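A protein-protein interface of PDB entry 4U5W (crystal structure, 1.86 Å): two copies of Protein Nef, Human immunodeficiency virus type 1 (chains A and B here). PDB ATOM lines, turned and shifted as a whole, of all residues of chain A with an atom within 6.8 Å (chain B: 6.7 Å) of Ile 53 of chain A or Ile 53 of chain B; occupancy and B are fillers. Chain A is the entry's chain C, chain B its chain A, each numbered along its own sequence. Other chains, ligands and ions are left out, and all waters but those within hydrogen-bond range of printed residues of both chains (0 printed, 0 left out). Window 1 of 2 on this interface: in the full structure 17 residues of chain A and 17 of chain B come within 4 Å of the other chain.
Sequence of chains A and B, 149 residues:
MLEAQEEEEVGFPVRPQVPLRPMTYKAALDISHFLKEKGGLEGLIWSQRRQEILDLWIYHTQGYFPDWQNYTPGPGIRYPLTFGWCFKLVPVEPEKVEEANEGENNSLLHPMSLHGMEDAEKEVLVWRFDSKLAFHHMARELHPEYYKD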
ATOM      1  N   PHE A  34      12.957  12.521   3.916  1.00  0.00           N
ATOM      2  CA  PHE A  34      11.931  12.039   4.835  1.00  0.00           C
ATOM      3  C   PHE A  34      11.181  10.856   4.225  1.00  0.00           C
ATOM      4  O   PHE A  34      10.939   9.835   4.880  1.00  0.00           O
ATOM      5  CB  PHE A  34      10.970  13.183   5.170  1.00  0.00           C
ATOM      6  CG  PHE A  34       9.867  12.800   6.111  1.00  0.00           C
ATOM      7  CD1 PHE A  34      10.076  12.799   7.478  1.00  0.00           C
ATOM      8  CD2 PHE A  34       8.614  12.475   5.627  1.00  0.00           C
ATOM      9  CE1 PHE A  34       9.055  12.459   8.348  1.00  0.00           C
ATOM     10  CE2 PHE A  34       7.589  12.130   6.491  1.00  0.00           C
ATOM     11  CZ  PHE A  34       7.815  12.126   7.851  1.00  0.00           C
ATOM     12  N   LEU A  35      10.830  10.989   2.953  1.00  0.00           N
ATOM     13  CA  LEU A  35       9.990  10.000   2.292  1.00  0.00           C
ATOM     14  C   LEU A  35      10.760   8.802   1.741  1.00  0.00           C
ATOM     15  O   LEU A  35      10.154   7.808   1.348  1.00  0.00           O
ATOM     16  CB  LEU A  35       9.205  10.670   1.169  1.00  0.00           C
ATOM     17  CG  LEU A  35       8.100  11.606   1.649  1.00  0.00           C
ATOM     18  CD1 LEU A  35       7.488  12.329   0.467  1.00  0.00           C
ATOM     19  CD2 LEU A  35       7.048  10.788   2.402  1.00  0.00           C
ATOM     20  N   GLY A  39       8.954   2.566   4.547  1.00  0.00           N
ATOM     21  CA  GLY A  39       7.558   2.832   4.838  1.00  0.00           C
ATOM     22  C   GLY A  39       7.045   4.043   4.088  1.00  0.00           C
ATOM     23  O   GLY A  39       5.863   4.366   4.157  1.00  0.00           O
ATOM     24  N   GLY A  40       7.938   4.712   3.362  1.00  0.00           N
ATOM     25  CA  GLY A  40       7.581   5.925   2.651  1.00  0.00           C
ATOM     26  C   GLY A  40       7.213   5.713   1.195  1.00  0.00           C
ATOM     27  O   GLY A  40       6.385   4.870   0.858  1.00  0.00           O
ATOM     28  N   GLN A  48      -1.817   8.785 -10.687  1.00  0.00           N
ATOM     29  CA  GLN A  48      -2.326  10.139 -10.455  1.00  0.00           C
ATOM     30  C   GLN A  48      -2.988  10.243  -9.074  1.00  0.00           C
ATOM     31  O   GLN A  48      -2.752  11.201  -8.334  1.00  0.00           O
ATOM     32  CB  GLN A  48      -3.318  10.539 -11.551  1.00  0.00           C
ATOM     33  CG  GLN A  48      -3.712  12.015 -11.526  1.00  0.00           C
ATOM     34  CD  GLN A  48      -2.531  12.935 -11.786  1.00  0.00           C
ATOM     35  OE1 GLN A  48      -1.807  12.772 -12.768  1.00  0.00           O
ATOM     36  NE2 GLN A  48      -2.332  13.909 -10.903  1.00  0.00           N
ATOM     37  N   ARG A  49      -3.802   9.250  -8.724  1.00  0.00           N
ATOM     38  CA  ARG A  49      -4.499   9.258  -7.435  1.00  0.00           C
ATOM     39  C   ARG A  49      -3.533   9.216  -6.251  1.00  0.00           C
ATOM     40  O   ARG A  49      -3.686   9.973  -5.284  1.00  0.00           O
ATOM     41  CB  ARG A  49      -5.479   8.084  -7.346  1.00  0.00           C
ATOM     42  CG  ARG A  49      -6.282   8.045  -6.046  1.00  0.00           C
ATOM     43  CD  ARG A  49      -7.262   9.217  -5.943  1.00  0.00           C
ATOM     44  NE  ARG A  49      -8.358   9.123  -6.909  1.00  0.00           N
ATOM     45  CZ  ARG A  49      -9.303  10.047  -7.067  1.00  0.00           C
ATOM     46  NH1 ARG A  49      -9.297  11.147  -6.320  1.00  0.00           N
ATOM     47  NH2 ARG A  49     -10.259   9.877  -7.969  1.00  0.00           N
ATOM     48  N   ARG A  50      -2.546   8.328  -6.306  1.00  0.00           N
ATOM     49  CA  ARG A  50      -1.546   8.261  -5.238  1.00  0.00           C
ATOM     50  C   ARG A  50      -0.759   9.559  -5.134  1.00  0.00           C
ATOM     51  O   ARG A  50      -0.468  10.037  -4.028  1.00  0.00           O
ATOM     52  CB  ARG A  50      -0.590   7.082  -5.461  1.00  0.00           C
ATOM     53  CG  ARG A  50      -1.276   5.723  -5.237  1.00  0.00           C
ATOM     54  CD  ARG A  50      -0.413   4.555  -5.704  1.00  0.00           C
ATOM     55  NE  ARG A  50      -1.124   3.284  -5.494  1.00  0.00           N
ATOM     56  CZ  ARG A  50      -0.567   2.083  -5.610  1.00  0.00           C
ATOM     57  NH1 ARG A  50       0.713   1.968  -5.946  1.00  0.00           N
ATOM     58  NH2 ARG A  50      -1.292   0.993  -5.396  1.00  0.00           N
ATOM     59  N   GLN A  51      -0.416  10.155  -6.268  1.00  0.00           N
ATOM     60  CA  GLN A  51       0.345  11.402  -6.188  1.00  0.00           C
ATOM     61  C   GLN A  51      -0.499  12.518  -5.577  1.00  0.00           C
ATOM     62  O   GLN A  51      -0.007  13.309  -4.767  1.00  0.00           O
ATOM     63  CB  GLN A  51       0.874  11.848  -7.552  1.00  0.00           C
ATOM     64  CG  GLN A  51       1.808  13.062  -7.391  1.00  0.00           C
ATOM     65  CD  GLN A  51       2.382  13.586  -8.685  1.00  0.00           C
ATOM     66  OE1 GLN A  51       2.720  12.823  -9.587  1.00  0.00           O
ATOM     67  NE2 GLN A  51       2.511  14.907  -8.779  1.00  0.00           N
ATOM     68  N   GLU A  52      -1.770  12.577  -5.957  1.00  0.00           N
ATOM     69  CA  GLU A  52      -2.663  13.604  -5.418  1.00  0.00           C
ATOM     70  C   GLU A  52      -2.869  13.436  -3.920  1.00  0.00           C
ATOM     71  O   GLU A  52      -2.943  14.424  -3.186  1.00  0.00           O
ATOM     72  CB  GLU A  52      -4.009  13.583  -6.142  1.00  0.00           C
ATOM     73  CG  GLU A  52      -3.940  14.159  -7.551  1.00  0.00           C
ATOM     74  CD  GLU A  52      -5.249  14.033  -8.307  1.00  0.00           C
ATOM     75  OE1 GLU A  52      -6.156  13.324  -7.822  1.00  0.00           O
ATOM     76  OE2 GLU A  52      -5.366  14.643  -9.392  1.00  0.00           O
ATOM     77  N   ILE A  53      -2.975  12.190  -3.464  1.00  0.00           N
ATOM     78  CA  ILE A  53      -3.142  11.931  -2.033  1.00  0.00           C
ATOM     79  C   ILE A  53      -1.895  12.402  -1.275  1.00  0.00           C
ATOM     80  O   ILE A  53      -1.996  13.108  -0.274  1.00  0.00           O
ATOM     81  CB  ILE A  53      -3.405  10.439  -1.742  1.00  0.00           C
ATOM     82  CG1 ILE A  53      -4.815  10.053  -2.196  1.00  0.00           C
ATOM     83  CG2 ILE A  53      -3.262  10.155  -0.243  1.00  0.00           C
ATOM     84  CD1 ILE A  53      -5.102   8.560  -2.117  1.00  0.00           C
ATOM     85  N   LEU A  54      -0.720  12.031  -1.770  1.00  0.00           N
ATOM     86  CA  LEU A  54       0.533  12.516  -1.194  1.00  0.00           C
ATOM     87  C   LEU A  54       0.633  14.050  -1.175  1.00  0.00           C
ATOM     88  O   LEU A  54       1.034  14.645  -0.172  1.00  0.00           O
ATOM     89  CB  LEU A  54       1.727  11.948  -1.966  1.00  0.00           C
ATOM     90  CG  LEU A  54       3.093  12.439  -1.493  1.00  0.00           C
ATOM     91  CD1 LEU A  54       3.385  11.943  -0.085  1.00  0.00           C
ATOM     92  CD2 LEU A  54       4.171  11.986  -2.471  1.00  0.00           C
ATOM     93  N   ASP A  55       0.282  14.685  -2.285  1.00  0.00           N
ATOM     94  CA  ASP A  55       0.420  16.132  -2.393  1.00  0.00           C
ATOM     95  C   ASP A  55      -0.540  16.854  -1.452  1.00  0.00           C
ATOM     96  O   ASP A  55      -0.191  17.883  -0.874  1.00  0.00           O
ATOM     97  CB  ASP A  55       0.207  16.584  -3.836  1.00  0.00           C
ATOM     98  CG  ASP A  55       1.425  16.308  -4.709  1.00  0.00           C
ATOM     99  OD1 ASP A  55       2.509  16.050  -4.143  1.00  0.00           O
ATOM    100  OD2 ASP A  55       1.312  16.356  -5.953  1.00  0.00           O
ATOM    101  N   LEU A  56      -1.737  16.306  -1.280  1.00  0.00           N
ATOM    102  CA  LEU A  56      -2.696  16.875  -0.340  1.00  0.00           C
ATOM    103  C   LEU A  56      -2.154  16.777   1.087  1.00  0.00           C
ATOM    104  O   LEU A  56      -2.282  17.719   1.875  1.00  0.00           O
ATOM    105  CB  LEU A  56      -4.055  16.169  -0.464  1.00  0.00           C
ATOM    106  CG  LEU A  56      -5.253  16.691   0.348  1.00  0.00           C
ATOM    107  CD1 LEU A  56      -5.259  16.168   1.780  1.00  0.00           C
ATOM    108  CD2 LEU A  56      -5.291  18.215   0.336  1.00  0.00           C
ATOM    109  N   TRP A  57      -1.563  15.634   1.425  1.00  0.00           N
ATOM    110  CA  TRP A  57      -1.022  15.439   2.762  1.00  0.00           C
ATOM    111  C   TRP A  57       0.117  16.430   3.027  1.00  0.00           C
ATOM    112  O   TRP A  57       0.191  17.030   4.102  1.00  0.00           O
ATOM    113  CB  TRP A  57      -0.538  14.003   2.939  1.00  0.00           C
ATOM    114  CG  TRP A  57       0.117  13.719   4.255  1.00  0.00           C
ATOM    115  CD1 TRP A  57      -0.503  13.434   5.434  1.00  0.00           C
ATOM    116  CD2 TRP A  57       1.528  13.661   4.517  1.00  0.00           C
ATOM    117  NE1 TRP A  57       0.432  13.212   6.418  1.00  0.00           N
ATOM    118  CE2 TRP A  57       1.683  13.348   5.881  1.00  0.00           C
ATOM    119  CE3 TRP A  57       2.668  13.845   3.732  1.00  0.00           C
ATOM    120  CZ2 TRP A  57       2.935  13.219   6.479  1.00  0.00           C
ATOM    121  CZ3 TRP A  57       3.911  13.719   4.327  1.00  0.00           C
ATOM    122  CH2 TRP A  57       4.033  13.410   5.688  1.00  0.00           C
ATOM    123  N   ILE A  58       1.003  16.613   2.048  1.00  0.00           N
ATOM    124  CA  ILE A  58       2.090  17.581   2.205  1.00  0.00           C
ATOM    125  C   ILE A  58       1.536  19.004   2.346  1.00  0.00           C
ATOM    126  O   ILE A  58       1.980  19.786   3.202  1.00  0.00           O
ATOM    127  CB  ILE A  58       3.080  17.502   1.031  1.00  0.00           C
ATOM    128  CG1 ILE A  58       3.845  16.176   1.115  1.00  0.00           C
ATOM    129  CG2 ILE A  58       4.055  18.702   1.061  1.00  0.00           C
ATOM    130  CD1 ILE A  58       4.759  15.901  -0.062  1.00  0.00           C
ATOM    131  N   LEU B  35     -11.499   2.986  -3.675  1.00  0.00           N
ATOM    132  CA  LEU B  35     -10.049   2.826  -3.591  1.00  0.00           C
ATOM    133  C   LEU B  35      -9.559   1.497  -4.159  1.00  0.00           C
ATOM    134  O   LEU B  35      -8.356   1.256  -4.219  1.00  0.00           O
ATOM    135  CB  LEU B  35      -9.597   2.969  -2.139  1.00  0.00           C
ATOM    136  CG  LEU B  35      -9.716   4.374  -1.538  1.00  0.00           C
ATOM    137  CD1 LEU B  35      -9.334   4.347  -0.080  1.00  0.00           C
ATOM    138  CD2 LEU B  35      -8.809   5.352  -2.302  1.00  0.00           C
ATOM    139  N   GLY B  39      -4.513   1.832  -9.416  1.00  0.00           N
ATOM    140  CA  GLY B  39      -3.903   3.103  -9.081  1.00  0.00           C
ATOM    141  C   GLY B  39      -4.381   3.584  -7.726  1.00  0.00           C
ATOM    142  O   GLY B  39      -3.954   4.631  -7.243  1.00  0.00           O
ATOM    143  N   GLY B  40      -5.273   2.812  -7.108  1.00  0.00           N
ATOM    144  CA  GLY B  40      -5.775   3.149  -5.789  1.00  0.00           C
ATOM    145  C   GLY B  40      -4.980   2.482  -4.682  1.00  0.00           C
ATOM    146  O   GLY B  40      -3.757   2.394  -4.740  1.00  0.00           O
ATOM    147  N   GLN B  48       2.716   2.069   8.541  1.00  0.00           N
ATOM    148  CA  GLN B  48       2.018   2.998   9.426  1.00  0.00           C
ATOM    149  C   GLN B  48       1.888   4.372   8.770  1.00  0.00           C
ATOM    150  O   GLN B  48       0.821   4.997   8.796  1.00  0.00           O
ATOM    151  CB  GLN B  48       2.760   3.110  10.764  1.00  0.00           C
ATOM    152  CG  GLN B  48       2.012   3.891  11.830  1.00  0.00           C
ATOM    153  CD  GLN B  48       0.672   3.272  12.165  1.00  0.00           C
ATOM    154  OE1 GLN B  48       0.548   2.052  12.273  1.00  0.00           O
ATOM    155  NE2 GLN B  48      -0.344   4.111  12.325  1.00  0.00           N
ATOM    156  N   ARG B  49       2.980   4.831   8.167  1.00  0.00           N
ATOM    157  CA  ARG B  49       3.008   6.146   7.536  1.00  0.00           C
ATOM    158  C   ARG B  49       2.022   6.233   6.376  1.00  0.00           C
ATOM    159  O   ARG B  49       1.298   7.230   6.230  1.00  0.00           O
ATOM    160  CB  ARG B  49       4.425   6.474   7.049  1.00  0.00           C
ATOM    161  CG  ARG B  49       4.543   7.812   6.332  1.00  0.00           C
ATOM    162  CD  ARG B  49       4.401   8.992   7.293  1.00  0.00           C
ATOM    163  NE  ARG B  49       5.521   9.090   8.228  1.00  0.00           N
ATOM    164  CZ  ARG B  49       5.600   9.978   9.215  1.00  0.00           C
ATOM    165  NH1 ARG B  49       4.623  10.857   9.406  1.00  0.00           N
ATOM    166  NH2 ARG B  49       6.658   9.989  10.016  1.00  0.00           N
ATOM    167  N   ARG B  50       1.995   5.196   5.549  1.00  0.00           N
ATOM    168  CA  ARG B  50       1.087   5.163   4.408  1.00  0.00           C
ATOM    169  C   ARG B  50      -0.364   5.149   4.869  1.00  0.00           C
ATOM    170  O   ARG B  50      -1.230   5.805   4.279  1.00  0.00           O
ATOM    171  CB  ARG B  50       1.387   3.951   3.530  1.00  0.00           C
ATOM    172  CG  ARG B  50       2.705   4.083   2.764  1.00  0.00           C
ATOM    173  CD  ARG B  50       3.164   2.739   2.185  1.00  0.00           C
ATOM    174  NE  ARG B  50       4.562   2.800   1.766  1.00  0.00           N
ATOM    175  CZ  ARG B  50       5.330   1.743   1.527  1.00  0.00           C
ATOM    176  NH1 ARG B  50       6.593   1.921   1.160  1.00  0.00           N
ATOM    177  NH2 ARG B  50       4.843   0.512   1.654  1.00  0.00           N
ATOM    178  N   GLN B  51      -0.638   4.411   5.933  1.00  0.00           N
ATOM    179  CA  GLN B  51      -2.000   4.362   6.440  1.00  0.00           C
ATOM    180  C   GLN B  51      -2.417   5.708   7.024  1.00  0.00           C
ATOM    181  O   GLN B  51      -3.563   6.129   6.869  1.00  0.00           O
ATOM    182  CB  GLN B  51      -2.160   3.274   7.492  1.00  0.00           C
ATOM    183  CG  GLN B  51      -3.621   3.055   7.865  1.00  0.00           C
ATOM    184  CD  GLN B  51      -3.800   2.144   9.054  1.00  0.00           C
ATOM    185  OE1 GLN B  51      -3.291   1.020   9.076  1.00  0.00           O
ATOM    186  NE2 GLN B  51      -4.534   2.618  10.050  1.00  0.00           N
ATOM    187  N   GLU B  52      -1.493   6.377   7.706  1.00  0.00           N
ATOM    188  CA  GLU B  52      -1.827   7.652   8.328  1.00  0.00           C
ATOM    189  C   GLU B  52      -2.063   8.710   7.259  1.00  0.00           C
ATOM    190  O   GLU B  52      -2.934   9.556   7.406  1.00  0.00           O
ATOM    191  CB  GLU B  52      -0.726   8.092   9.303  1.00  0.00           C
ATOM    192  CG  GLU B  52      -0.729   7.285  10.606  1.00  0.00           C
ATOM    193  CD  GLU B  52       0.453   7.589  11.509  1.00  0.00           C
ATOM    194  OE1 GLU B  52       1.315   8.408  11.121  1.00  0.00           O
ATOM    195  OE2 GLU B  52       0.521   7.004  12.612  1.00  0.00           O
ATOM    196  N   ILE B  53      -1.292   8.651   6.176  1.00  0.00           N
ATOM    197  CA  ILE B  53      -1.463   9.591   5.072  1.00  0.00           C
ATOM    198  C   ILE B  53      -2.849   9.411   4.445  1.00  0.00           C
ATOM    199  O   ILE B  53      -3.588  10.383   4.245  1.00  0.00           O
ATOM    200  CB  ILE B  53      -0.341   9.412   4.013  1.00  0.00           C
ATOM    201  CG1 ILE B  53       0.984   9.953   4.560  1.00  0.00           C
ATOM    202  CG2 ILE B  53      -0.680  10.137   2.720  1.00  0.00           C
ATOM    203  CD1 ILE B  53       2.170   9.685   3.652  1.00  0.00           C
ATOM    204  N   LEU B  54      -3.207   8.163   4.163  1.00  0.00           N
ATOM    205  CA  LEU B  54      -4.542   7.832   3.664  1.00  0.00           C
ATOM    206  C   LEU B  54      -5.658   8.323   4.583  1.00  0.00           C
ATOM    207  O   LEU B  54      -6.628   8.943   4.132  1.00  0.00           O
ATOM    208  CB  LEU B  54      -4.673   6.320   3.481  1.00  0.00           C
ATOM    209  CG  LEU B  54      -6.049   5.834   3.023  1.00  0.00           C
ATOM    210  CD1 LEU B  54      -6.341   6.338   1.618  1.00  0.00           C
ATOM    211  CD2 LEU B  54      -6.108   4.318   3.085  1.00  0.00           C
ATOM    212  N   ASP B  55      -5.521   8.043   5.874  1.00  0.00           N
ATOM    213  CA  ASP B  55      -6.530   8.478   6.844  1.00  0.00           C
ATOM    214  C   ASP B  55      -6.676   9.998   6.890  1.00  0.00           C
ATOM    215  O   ASP B  55      -7.787  10.513   7.058  1.00  0.00           O
ATOM    216  CB  ASP B  55      -6.195   7.946   8.237  1.00  0.00           C
ATOM    217  CG  ASP B  55      -6.565   6.479   8.402  1.00  0.00           C
ATOM    218  OD1 ASP B  55      -7.329   5.958   7.561  1.00  0.00           O
ATOM    219  OD2 ASP B  55      -6.098   5.848   9.371  1.00  0.00           O
ATOM    220  N   LEU B  56      -5.565  10.718   6.736  1.00  0.00           N
ATOM    221  CA  LEU B  56      -5.623  12.175   6.750  1.00  0.00           C
ATOM    222  C   LEU B  56      -6.351  12.671   5.508  1.00  0.00           C
ATOM    223  O   LEU B  56      -7.148  13.606   5.571  1.00  0.00           O
ATOM    224  CB  LEU B  56      -4.208  12.777   6.833  1.00  0.00           C
ATOM    225  CG  LEU B  56      -4.025  14.294   6.992  1.00  0.00           C
ATOM    226  CD1 LEU B  56      -4.125  15.040   5.660  1.00  0.00           C
ATOM    227  CD2 LEU B  56      -5.016  14.853   8.010  1.00  0.00           C
ATOM    228  N   TRP B  57      -6.055  12.058   4.370  1.00  0.00           N
ATOM    229  CA  TRP B  57      -6.687  12.457   3.124  1.00  0.00           C
ATOM    230  C   TRP B  57      -8.205  12.254   3.205  1.00  0.00           C
ATOM    231  O   TRP B  57      -8.987  13.128   2.825  1.00  0.00           O
ATOM    232  CB  TRP B  57      -6.085  11.668   1.958  1.00  0.00           C
ATOM    233  CG  TRP B  57      -6.731  11.936   0.641  1.00  0.00           C
ATOM    234  CD1 TRP B  57      -6.524  13.010  -0.168  1.00  0.00           C
ATOM    235  CD2 TRP B  57      -7.680  11.100  -0.033  1.00  0.00           C
ATOM    236  NE1 TRP B  57      -7.295  12.900  -1.304  1.00  0.00           N
ATOM    237  CE2 TRP B  57      -8.015  11.738  -1.242  1.00  0.00           C
ATOM    238  CE3 TRP B  57      -8.282   9.877   0.270  1.00  0.00           C
ATOM    239  CZ2 TRP B  57      -8.920  11.192  -2.151  1.00  0.00           C
ATOM    240  CZ3 TRP B  57      -9.185   9.337  -0.631  1.00  0.00           C
ATOM    241  CH2 TRP B  57      -9.496   9.998  -1.827  1.00  0.00           C
ATOM    242  N   ILE B  58      -8.616  11.099   3.717  1.00  0.00           N
ATOM    243  CA  ILE B  58     -10.034  10.801   3.910  1.00  0.00           C
ATOM    244  C   ILE B  58     -10.693  11.796   4.861  1.00  0.00           C
ATOM    245  O   ILE B  58     -11.789  12.287   4.599  1.00  0.00           O
ATOM    246  CB  ILE B  58     -10.203   9.368   4.428  1.00  0.00           C
ATOM    247  CG1 ILE B  58      -9.840   8.398   3.300  1.00  0.00           C
ATOM    248  CG2 ILE B  58     -11.638   9.121   4.920  1.00  0.00           C
ATOM    249  CD1 ILE B  58      -9.722   6.938   3.731  1.00  0.00           C
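Printed residues of chain B that touch a printed residue of chain A: Gly 39, Gly 40, Arg 49, Arg 50, Ile 53, Leu 56 and Trp 57.
Hydrophobic or aromatic side chains of chain B that line the printed part of chain A: Ile 53, Leu 56 and Trp 57.
Of the 15 printed residues of chain A, 8 touch a printed residue of chain B.
Hydrophobic or aromatic side chains of chain A within 4 Å of the printed part of chain B: Phe 34, Ile 53, Leu 56 and Trp 57.
Among the printed residues, 12 pairs touch across the chains.
The backbone carbonyl oxygen (O) of Gly 40 of chain B lies within hydrogen-bond range of the guanidinium group (NE) of Arg 50 of chain A (2.9 Å).
The guanidinium group (NE) of Arg 50 of chain B sits at hydrogen-bond distance from the backbone carbonyl oxygen (O) of Gly 39 of chain A (3.1 Å).
The guanidinium group (NE) of Arg 50 of chain B sits at hydrogen-bond distance from the backbone carbonyl oxygen (O) of Gly 40 of chain A, 2.9 Å away.
Gly 39 of chain A touches Arg 49 of chain B, and with the chains exchanged Arg 49 of chain A touches Gly 39 of chain B.
Gly 39 of chain A touches Arg 50 of chain B, and with the chains exchanged Arg 50 of chain A touches Gly 39 of chain B.
Gly 40 of chain A touches Arg 50 of chain B, and with the chains exchanged Arg 50 of chain A touches Gly 40 of chain B.
Leu 56 of chain A touches Trp 57 of chain B, and with the chains exchanged Trp 57 of chain A touches Leu 56 of chain B.
Positions printed for both chains: 35, 39, 40, 48, 49, 50, 51, 52, 53, 54, 55, 56, 57 and 58.
Among the printed residues, pairs that only touch across the chains: Phe 34 of chain A with Arg 49 of chain B, Gly 39 of chain A with Arg 49 of chain B, Arg 49 of chain A with Gly 39 of chain B, Arg 50 of chain A with Gly 39 of chain B, Ile 53 of chain A with Ile 53 of chain B, Ile 53 of chain A with Trp 57 of chain B, Leu 56 of chain A with Trp 57 of chain B, Trp 57 of chain A with Ile 53 of chain B and Trp 57 of chain A with Leu 56 of chain B.
Of chain B, only Ile 53 (3.9 Å) and Trp 57 (3.7 Å) come within 4 Å of Ile 53 of chain A.
Ile 53 of chain B touches two residues of chain A.
Printed residues of chain A within 4 Å of Leu 56 of chain B: Trp 57 (3.9 Å).
Printed residues of chain B within 4 Å of Arg 49 of chain A: Gly 39.
Of the printed residues of chain B, Gly 40 of chain A touches Arg 50 (2.9 Å).
Of the printed residues of chain B, Trp 57 of chain A touches Ile 53 and Leu 56.
Glu 52 of chain A touches none of the printed residues of chain B.
Ile 58 of chain B touches none of the printed residues of chain A.
The nearest residue of chain A that does not touch Ile 53 of chain B is Leu 54 of chain A (4.5 Å).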
